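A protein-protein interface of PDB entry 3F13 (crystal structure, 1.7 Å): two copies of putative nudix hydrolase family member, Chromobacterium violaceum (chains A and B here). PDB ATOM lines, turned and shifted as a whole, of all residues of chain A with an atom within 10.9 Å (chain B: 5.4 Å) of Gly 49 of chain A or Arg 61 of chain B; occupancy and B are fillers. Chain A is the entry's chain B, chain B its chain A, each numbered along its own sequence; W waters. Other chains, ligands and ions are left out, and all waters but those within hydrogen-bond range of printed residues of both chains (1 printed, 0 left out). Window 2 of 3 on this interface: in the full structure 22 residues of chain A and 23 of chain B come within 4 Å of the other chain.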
ATOM      1  N   ARG A  17     -27.394  18.320  -3.335  1.00  0.00           N
ATOM      2  CA  ARG A  17     -27.279  19.609  -2.601  1.00  0.00           C
ATOM      3  C   ARG A  17     -28.133  20.681  -3.251  1.00  0.00           C
ATOM      4  O   ARG A  17     -28.002  20.938  -4.469  1.00  0.00           O
ATOM      5  CB  ARG A  17     -25.828  20.056  -2.555  1.00  0.00           C
ATOM      6  CG  ARG A  17     -24.896  19.144  -1.725  1.00  0.00           C
ATOM      7  CD  ARG A  17     -23.451  19.699  -1.766  1.00  0.00           C
ATOM      8  NE  ARG A  17     -23.002  19.824  -3.159  1.00  0.00           N
ATOM      9  CZ  ARG A  17     -22.553  20.940  -3.744  1.00  0.00           C
ATOM     10  NH1 ARG A  17     -22.205  20.901  -5.018  1.00  0.00           N
ATOM     11  NH2 ARG A  17     -22.400  22.087  -3.083  1.00  0.00           N
ATOM     12  N   LYS A  45     -30.573  23.111  -7.614  1.00  0.00           N
ATOM     13  CA  LYS A  45     -29.491  22.233  -7.305  1.00  0.00           C
ATOM     14  C   LYS A  45     -28.139  22.884  -7.579  1.00  0.00           C
ATOM     15  O   LYS A  45     -27.968  23.613  -8.568  1.00  0.00           O
ATOM     16  CB  LYS A  45     -29.636  20.948  -8.118  1.00  0.00           C
ATOM     17  CG  LYS A  45     -28.839  19.797  -7.569  1.00  0.00           C
ATOM     18  CD  LYS A  45     -28.954  18.574  -8.494  1.00  0.00           C
ATOM     19  CE  LYS A  45     -27.810  17.623  -8.249  1.00  0.00           C
ATOM     20  NZ  LYS A  45     -28.281  16.203  -8.403  1.00  0.00           N
ATOM     21  N   ALA A  46     -27.185  22.622  -6.701  1.00  0.00           N
ATOM     22  CA  ALA A  46     -25.804  23.100  -6.835  1.00  0.00           C
ATOM     23  C   ALA A  46     -25.003  22.244  -7.833  1.00  0.00           C
ATOM     24  O   ALA A  46     -25.137  21.031  -7.840  1.00  0.00           O
ATOM     25  CB  ALA A  46     -25.131  23.042  -5.496  1.00  0.00           C
ATOM     26  N   ASN A  47     -24.162  22.855  -8.655  1.00  0.00           N
ATOM     27  CA  ASN A  47     -23.334  22.033  -9.571  1.00  0.00           C
ATOM     28  C   ASN A  47     -22.143  21.481  -8.813  1.00  0.00           C
ATOM     29  O   ASN A  47     -21.763  22.005  -7.752  1.00  0.00           O
ATOM     30  CB  ASN A  47     -22.842  22.863 -10.755  1.00  0.00           C
ATOM     31  CG  ASN A  47     -23.968  23.386 -11.615  1.00  0.00           C
ATOM     32  OD1 ASN A  47     -23.953  24.549 -12.021  1.00  0.00           O
ATOM     33  ND2 ASN A  47     -24.946  22.538 -11.904  1.00  0.00           N
ATOM     34  N   ARG A  48     -21.551  20.408  -9.336  1.00  0.00           N
ATOM     35  CA  ARG A  48     -20.288  19.935  -8.790  1.00  0.00           C
ATOM     36  C   ARG A  48     -19.284  21.087  -8.767  1.00  0.00           C
ATOM     37  O   ARG A  48     -19.242  21.898  -9.685  1.00  0.00           O
ATOM     38  CB  ARG A  48     -19.748  18.786  -9.660  1.00  0.00           C
ATOM     39  CG  ARG A  48     -20.440  17.451  -9.449  1.00  0.00           C
ATOM     40  CD  ARG A  48     -19.943  16.462 -10.574  1.00  0.00           C
ATOM     41  NE  ARG A  48     -20.735  15.244 -10.613  1.00  0.00           N
ATOM     42  CZ  ARG A  48     -21.838  15.126 -11.340  1.00  0.00           C
ATOM     43  NH1 ARG A  48     -22.235  16.136 -12.111  1.00  0.00           N
ATOM     44  NH2 ARG A  48     -22.521  13.988 -11.327  1.00  0.00           N
ATOM     45  N   GLY A  49     -18.478  21.187  -7.721  1.00  0.00           N
ATOM     46  CA  GLY A  49     -17.529  22.281  -7.612  1.00  0.00           C
ATOM     47  C   GLY A  49     -18.095  23.614  -7.141  1.00  0.00           C
ATOM     48  O   GLY A  49     -17.340  24.569  -6.943  1.00  0.00           O
ATOM     49  N   GLU A  50     -19.416  23.680  -6.966  1.00  0.00           N
ATOM     50  CA  GLU A  50     -20.117  24.929  -6.669  1.00  0.00           C
ATOM     51  C   GLU A  50     -20.743  24.829  -5.290  1.00  0.00           C
ATOM     52  O   GLU A  50     -21.542  23.922  -5.043  1.00  0.00           O
ATOM     53  CB  GLU A  50     -21.265  25.131  -7.667  1.00  0.00           C
ATOM     54  CG  GLU A  50     -21.989  26.461  -7.557  1.00  0.00           C
ATOM     55  CD  GLU A  50     -23.163  26.556  -8.522  1.00  0.00           C
ATOM     56  OE1 GLU A  50     -23.354  27.647  -9.124  1.00  0.00           O
ATOM     57  OE2 GLU A  50     -23.880  25.540  -8.685  1.00  0.00           O
ATOM     58  N   LEU A  51     -20.392  25.756  -4.399  1.00  0.00           N
ATOM     59  CA  LEU A  51     -21.041  25.828  -3.099  1.00  0.00           C
ATOM     60  C   LEU A  51     -22.530  26.170  -3.242  1.00  0.00           C
ATOM     61  O   LEU A  51     -22.942  26.802  -4.217  1.00  0.00           O
ATOM     62  CB  LEU A  51     -20.374  26.930  -2.287  1.00  0.00           C
ATOM     63  CG  LEU A  51     -18.900  26.667  -2.004  1.00  0.00           C
ATOM     64  CD1 LEU A  51     -18.236  27.926  -1.393  1.00  0.00           C
ATOM     65  CD2 LEU A  51     -18.728  25.467  -1.067  1.00  0.00           C
ATOM     66  N   ARG A  52     -23.342  25.747  -2.285  1.00  0.00           N
ATOM     67  CA  ARG A  52     -24.761  26.128  -2.277  1.00  0.00           C
ATOM     68  C   ARG A  52     -24.964  27.637  -2.246  1.00  0.00           C
ATOM     69  O   ARG A  52     -25.904  28.159  -2.833  1.00  0.00           O
ATOM     70  CB  ARG A  52     -25.509  25.404  -1.150  1.00  0.00           C
ATOM     71  CG  ARG A  52     -25.907  24.017  -1.644  1.00  0.00           C
ATOM     72  CD  ARG A  52     -26.356  23.070  -0.563  1.00  0.00           C
ATOM     73  NE  ARG A  52     -25.225  22.546   0.188  1.00  0.00           N
ATOM     74  CZ  ARG A  52     -25.334  21.608   1.141  1.00  0.00           C
ATOM     75  NH1 ARG A  52     -24.263  21.231   1.791  1.00  0.00           N
ATOM     76  NH2 ARG A  52     -26.508  21.021   1.422  1.00  0.00           N
ATOM     77  N   SER A  53     -24.055  28.351  -1.598  1.00  0.00           N
ATOM     78  CA  SER A  53     -24.254  29.791  -1.526  1.00  0.00           C
ATOM     79  C   SER A  53     -24.003  30.365  -2.919  1.00  0.00           C
ATOM     80  O   SER A  53     -24.652  31.320  -3.298  1.00  0.00           O
ATOM     81  CB  SER A  53     -23.299  30.411  -0.520  1.00  0.00           C
ATOM     82  OG  SER A  53     -21.981  29.970  -0.779  1.00  0.00           O
ATOM     83  N   GLN A  54     -23.135  29.725  -3.725  1.00  0.00           N
ATOM     84  CA  GLN A  54     -22.911  30.174  -5.105  1.00  0.00           C
ATOM     85  C   GLN A  54     -24.120  29.838  -5.968  1.00  0.00           C
ATOM     86  O   GLN A  54     -24.596  30.641  -6.775  1.00  0.00           O
ATOM     87  CB  GLN A  54     -21.707  29.464  -5.721  1.00  0.00           C
ATOM     88  CG  GLN A  54     -20.396  29.993  -5.245  1.00  0.00           C
ATOM     89  CD  GLN A  54     -19.234  29.203  -5.830  1.00  0.00           C
ATOM     90  OE1 GLN A  54     -18.845  28.171  -5.293  1.00  0.00           O
ATOM     91  NE2 GLN A  54     -18.682  29.692  -6.938  1.00  0.00           N
ATOM     92  N   ALA A  55     -24.584  28.621  -5.824  1.00  0.00           N
ATOM     93  CA  ALA A  55     -25.722  28.193  -6.578  1.00  0.00           C
ATOM     94  C   ALA A  55     -26.939  29.076  -6.244  1.00  0.00           C
ATOM     95  O   ALA A  55     -27.745  29.401  -7.109  1.00  0.00           O
ATOM     96  CB  ALA A  55     -25.984  26.734  -6.275  1.00  0.00           C
ATOM     97  N   ARG A  58     -26.868  32.335  -8.322  1.00  0.00           N
ATOM     98  CA  ARG A  58     -27.102  32.013  -9.719  1.00  0.00           C
ATOM     99  C   ARG A  58     -28.583  31.712  -9.954  1.00  0.00           C
ATOM    100  O   ARG A  58     -29.231  32.273 -10.848  1.00  0.00           O
ATOM    101  CB  ARG A  58     -26.237  30.813 -10.107  1.00  0.00           C
ATOM    102  CG  ARG A  58     -26.605  30.133 -11.444  1.00  0.00           C
ATOM    103  CD  ARG A  58     -25.622  28.998 -11.777  1.00  0.00           C
ATOM    104  NE  ARG A  58     -25.608  27.895 -10.801  1.00  0.00           N
ATOM    105  CZ  ARG A  58     -26.570  26.983 -10.705  1.00  0.00           C
ATOM    106  NH1 ARG A  58     -27.627  27.054 -11.516  1.00  0.00           N
ATOM    107  NH2 ARG A  58     -26.496  26.014  -9.790  1.00  0.00           N
ATOM    108  N   LEU B  56     -17.060  36.746  -5.576  1.00  0.00           N
ATOM    109  CA  LEU B  56     -16.437  36.815  -4.271  1.00  0.00           C
ATOM    110  C   LEU B  56     -16.398  35.439  -3.582  1.00  0.00           C
ATOM    111  O   LEU B  56     -15.367  35.038  -3.027  1.00  0.00           O
ATOM    112  CB  LEU B  56     -17.181  37.823  -3.374  1.00  0.00           C
ATOM    113  CG  LEU B  56     -16.307  38.054  -2.134  1.00  0.00           C
ATOM    114  CD1 LEU B  56     -14.916  38.415  -2.580  1.00  0.00           C
ATOM    115  CD2 LEU B  56     -16.863  39.160  -1.305  1.00  0.00           C
ATOM    116  N   ILE B  57     -17.504  34.705  -3.654  1.00  0.00           N
ATOM    117  CA  ILE B  57     -17.544  33.410  -2.981  1.00  0.00           C
ATOM    118  C   ILE B  57     -16.535  32.465  -3.634  1.00  0.00           C
ATOM    119  O   ILE B  57     -15.813  31.748  -2.959  1.00  0.00           O
ATOM    120  CB  ILE B  57     -18.920  32.772  -3.080  1.00  0.00           C
ATOM    121  CG1 ILE B  57     -19.927  33.593  -2.270  1.00  0.00           C
ATOM    122  CG2 ILE B  57     -18.827  31.402  -2.460  1.00  0.00           C
ATOM    123  CD1 ILE B  57     -21.405  33.248  -2.589  1.00  0.00           C
ATOM    124  N   ARG B  58     -16.491  32.493  -4.956  1.00  0.00           N
ATOM    125  CA  ARG B  58     -15.553  31.678  -5.727  1.00  0.00           C
ATOM    126  C   ARG B  58     -14.103  31.994  -5.369  1.00  0.00           C
ATOM    127  O   ARG B  58     -13.265  31.113  -5.107  1.00  0.00           O
ATOM    128  CB  ARG B  58     -15.754  31.952  -7.209  1.00  0.00           C
ATOM    129  CG  ARG B  58     -14.696  31.281  -8.040  1.00  0.00           C
ATOM    130  CD  ARG B  58     -15.000  31.403  -9.524  1.00  0.00           C
ATOM    131  NE  ARG B  58     -15.360  32.746  -9.986  1.00  0.00           N
ATOM    132  CZ  ARG B  58     -14.481  33.666 -10.357  1.00  0.00           C
ATOM    133  NH1 ARG B  58     -13.180  33.423 -10.274  1.00  0.00           N
ATOM    134  NH2 ARG B  58     -14.898  34.847 -10.790  1.00  0.00           N
ATOM    135  N   GLU B  59     -13.807  33.273  -5.302  1.00  0.00           N
ATOM    136  CA  GLU B  59     -12.427  33.688  -5.168  1.00  0.00           C
ATOM    137  C   GLU B  59     -11.918  33.558  -3.751  1.00  0.00           C
ATOM    138  O   GLU B  59     -10.746  33.216  -3.526  1.00  0.00           O
ATOM    139  CB  GLU B  59     -12.227  35.083  -5.730  1.00  0.00           C
ATOM    140  CG  GLU B  59     -12.301  35.093  -7.260  1.00  0.00           C
ATOM    141  CD  GLU B  59     -12.444  36.465  -7.855  1.00  0.00           C
ATOM    142  OE1 GLU B  59     -12.906  37.400  -7.146  1.00  0.00           O
ATOM    143  OE2 GLU B  59     -12.099  36.595  -9.071  1.00  0.00           O
ATOM    144  N   ILE B  60     -12.760  33.851  -2.769  1.00  0.00           N
ATOM    145  CA  ILE B  60     -12.341  33.588  -1.404  1.00  0.00           C
ATOM    146  C   ILE B  60     -12.048  32.090  -1.206  1.00  0.00           C
ATOM    147  O   ILE B  60     -11.043  31.703  -0.590  1.00  0.00           O
ATOM    148  CB  ILE B  60     -13.395  34.047  -0.423  1.00  0.00           C
ATOM    149  CG1 ILE B  60     -13.536  35.582  -0.488  1.00  0.00           C
ATOM    150  CG2 ILE B  60     -13.084  33.488   0.984  1.00  0.00           C
ATOM    151  CD1 ILE B  60     -12.270  36.318  -0.188  1.00  0.00           C
ATOM    152  N   ARG B  61     -12.914  31.224  -1.726  1.00  0.00           N
ATOM    153  CA  ARG B  61     -12.598  29.804  -1.645  1.00  0.00           C
ATOM    154  C   ARG B  61     -11.274  29.450  -2.311  1.00  0.00           C
ATOM    155  O   ARG B  61     -10.463  28.742  -1.722  1.00  0.00           O
ATOM    156  CB  ARG B  61     -13.722  28.900  -2.158  1.00  0.00           C
ATOM    157  CG  ARG B  61     -13.456  27.478  -1.779  1.00  0.00           C
ATOM    158  CD  ARG B  61     -14.561  26.523  -2.243  1.00  0.00           C
ATOM    159  NE  ARG B  61     -14.093  25.167  -1.999  1.00  0.00           N
ATOM    160  CZ  ARG B  61     -14.304  24.144  -2.820  1.00  0.00           C
ATOM    161  NH1 ARG B  61     -15.001  24.315  -3.940  1.00  0.00           N
ATOM    162  NH2 ARG B  61     -13.807  22.949  -2.505  1.00  0.00           N
ATOM    163  N   GLU B  62     -11.045  29.946  -3.518  1.00  0.00           N
ATOM    164  CA  GLU B  62      -9.784  29.685  -4.215  1.00  0.00           C
ATOM    165  C   GLU B  62      -8.557  30.159  -3.435  1.00  0.00           C
ATOM    166  O   GLU B  62      -7.542  29.477  -3.407  1.00  0.00           O
ATOM    167  CB  GLU B  62      -9.774  30.256  -5.655  1.00  0.00           C
ATOM    168  N   GLU B  63      -8.653  31.312  -2.782  1.00  0.00           N
ATOM    169  CA  GLU B  63      -7.470  31.957  -2.195  1.00  0.00           C
ATOM    170  C   GLU B  63      -7.170  31.408  -0.802  1.00  0.00           C
ATOM    171  O   GLU B  63      -6.036  31.442  -0.365  1.00  0.00           O
ATOM    172  CB  GLU B  63      -7.671  33.497  -2.130  1.00  0.00           C
ATOM    173  CG  GLU B  63      -7.849  34.104  -3.526  1.00  0.00           C
ATOM    174  CD  GLU B  63      -8.457  35.524  -3.580  1.00  0.00           C
ATOM    175  OE1 GLU B  63      -8.849  36.125  -2.547  1.00  0.00           O
ATOM    176  OE2 GLU B  63      -8.532  36.057  -4.716  1.00  0.00           O
ATOM    177  N   THR B  64      -8.187  30.917  -0.102  1.00  0.00           N
ATOM    178  CA  THR B  64      -8.036  30.617   1.324  1.00  0.00           C
ATOM    179  C   THR B  64      -8.716  29.339   1.773  1.00  0.00           C
ATOM    180  O   THR B  64      -8.580  28.961   2.930  1.00  0.00           O
ATOM    181  CB  THR B  64      -8.702  31.695   2.216  1.00  0.00           C
ATOM    182  OG1 THR B  64     -10.139  31.561   2.144  1.00  0.00           O
ATOM    183  CG2 THR B  64      -8.272  33.144   1.813  1.00  0.00           C
ATOM    184  N   GLY B  65      -9.515  28.731   0.904  1.00  0.00           N
ATOM    185  CA  GLY B  65     -10.277  27.541   1.277  1.00  0.00           C
ATOM    186  C   GLY B  65     -11.539  27.797   2.088  1.00  0.00           C
ATOM    187  O   GLY B  65     -12.323  26.871   2.379  1.00  0.00           O
ATOM    188  N   LEU B  66     -11.762  29.049   2.480  1.00  0.00           N
ATOM    189  CA  LEU B  66     -12.976  29.337   3.252  1.00  0.00           C
ATOM    190  C   LEU B  66     -14.207  29.201   2.351  1.00  0.00           C
ATOM    191  O   LEU B  66     -14.163  29.567   1.186  1.00  0.00           O
ATOM    192  CB  LEU B  66     -12.916  30.737   3.856  1.00  0.00           C
ATOM    193  CG  LEU B  66     -11.937  30.933   5.025  1.00  0.00           C
ATOM    194  CD1 LEU B  66     -12.129  32.290   5.686  1.00  0.00           C
ATOM    195  CD2 LEU B  66     -12.175  29.817   6.056  1.00  0.00           C
ATOM    196  N   ARG B  67     -15.292  28.656   2.890  1.00  0.00           N
ATOM    197  CA  ARG B  67     -16.557  28.545   2.165  1.00  0.00           C
ATOM    198  C   ARG B  67     -17.556  29.564   2.747  1.00  0.00           C
ATOM    199  O   ARG B  67     -18.081  29.381   3.827  1.00  0.00           O
ATOM    200  CB  ARG B  67     -17.094  27.106   2.291  1.00  0.00           C
ATOM    201  CG  ARG B  67     -16.111  26.087   1.658  1.00  0.00           C
ATOM    202  CD  ARG B  67     -16.371  24.613   2.079  1.00  0.00           C
ATOM    203  NE  ARG B  67     -15.261  23.780   1.606  1.00  0.00           N
ATOM    204  CZ  ARG B  67     -15.225  22.446   1.657  1.00  0.00           C
ATOM    205  NH1 ARG B  67     -16.252  21.754   2.146  1.00  0.00           N
ATOM    206  NH2 ARG B  67     -14.149  21.807   1.199  1.00  0.00           N
ATOM    207  N   GLN B  98      -3.451  29.408  -0.262  1.00  0.00           N
ATOM    208  CA  GLN B  98      -3.878  28.476  -1.293  1.00  0.00           C
ATOM    209  C   GLN B  98      -3.475  29.025  -2.640  1.00  0.00           C
ATOM    210  O   GLN B  98      -3.429  30.238  -2.821  1.00  0.00           O
ATOM    211  CB  GLN B  98      -5.403  28.459  -1.310  1.00  0.00           C
ATOM    212  CG  GLN B  98      -6.002  27.120  -1.475  1.00  0.00           C
ATOM    213  CD  GLN B  98      -6.554  26.651  -0.174  1.00  0.00           C
ATOM    214  OE1 GLN B  98      -7.195  25.613  -0.102  1.00  0.00           O
ATOM    215  NE2 GLN B  98      -6.316  27.432   0.885  1.00  0.00           N
HETATM  216  O   HOH W   1     -16.676  26.367  -5.241  1.00  0.00           O
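1 position is printed for both chains.
Among the printed residues, pairs that only touch across the chains: Gln 54 of chain A with Ile 57 of chain B, Leu 51 of chain A with Ile 57 of chain B, Gln 54 of chain A with Arg 58 of chain B, Ser 53 of chain A with Ile 57 of chain B, Gly 49 of chain A with Arg 61 of chain B and Leu 51 of chain A with Arg 67 of chain B.
Gly 49 of chain A touches one residue of chain B.
Arg 61 of chain B touches one residue of chain A.
No residue of chain A comes within 4 Å of Glu 62 of chain B.
No residue of chain A comes within 4 Å of Thr 64 of chain B.
Printed residues of chain B within 4 Å of Leu 51 of chain A: Ile 57 (3.7 Å) and Arg 67 (3.8 Å).
Of the printed residues of chain A, Arg 58 of chain B touches Gln 54 (3.7 Å).
Of the printed residues of chain A, Ile 57 of chain B touches Leu 51, Ser 53 and Gln 54.
Of the printed residues of chain B, Gln 54 of chain A touches Ile 57 and Arg 58.
Of the printed residues of chain A, Arg 67 of chain B touches Leu 51 (3.8 Å).
Arg 58 of chain A touches none of the printed residues of chain B.
Glu 59 of chain B touches none of the printed residues of chain A.
The nearest printed residue of chain B that does not touch Gly 49 of chain A is Arg 58 of chain B (7.3 Å).
The nearest residue of chain A that does not touch Arg 61 of chain B is Leu 51 of chain A (4.02 Å).
The nearest printed residue of chain B that does not touch Gln 54 of chain A is Arg 61 of chain B (5.5 Å).
Water W1 lies within hydrogen-bond range of O of Gly 49 of chain A (2.6 Å), OE1 of Gln 54 of chain A (2.8 Å) and NH1 of Arg 61 of chain B (3.0 Å).
The guanidinium group of Arg 58 of chain B is in salt-bridge range of the side-chain carboxylate of Glu 59 of chain B (3.6 Å).
The side-chain amide oxygen of Gln 54 of chain A lies within hydrogen-bond range of the backbone NH of Leu 51 of chain A, 3.0 Å away.
Hydrophobic or aromatic side chains of chain A within 4 Å of the printed part of chain B: Leu 51.
Among the printed residues, 6 pairs touch across the chains.
Among the printed residues, no Asp or Glu carboxylate lies within 4 Å of a Lys or Arg side-chain nitrogen of the other chain.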
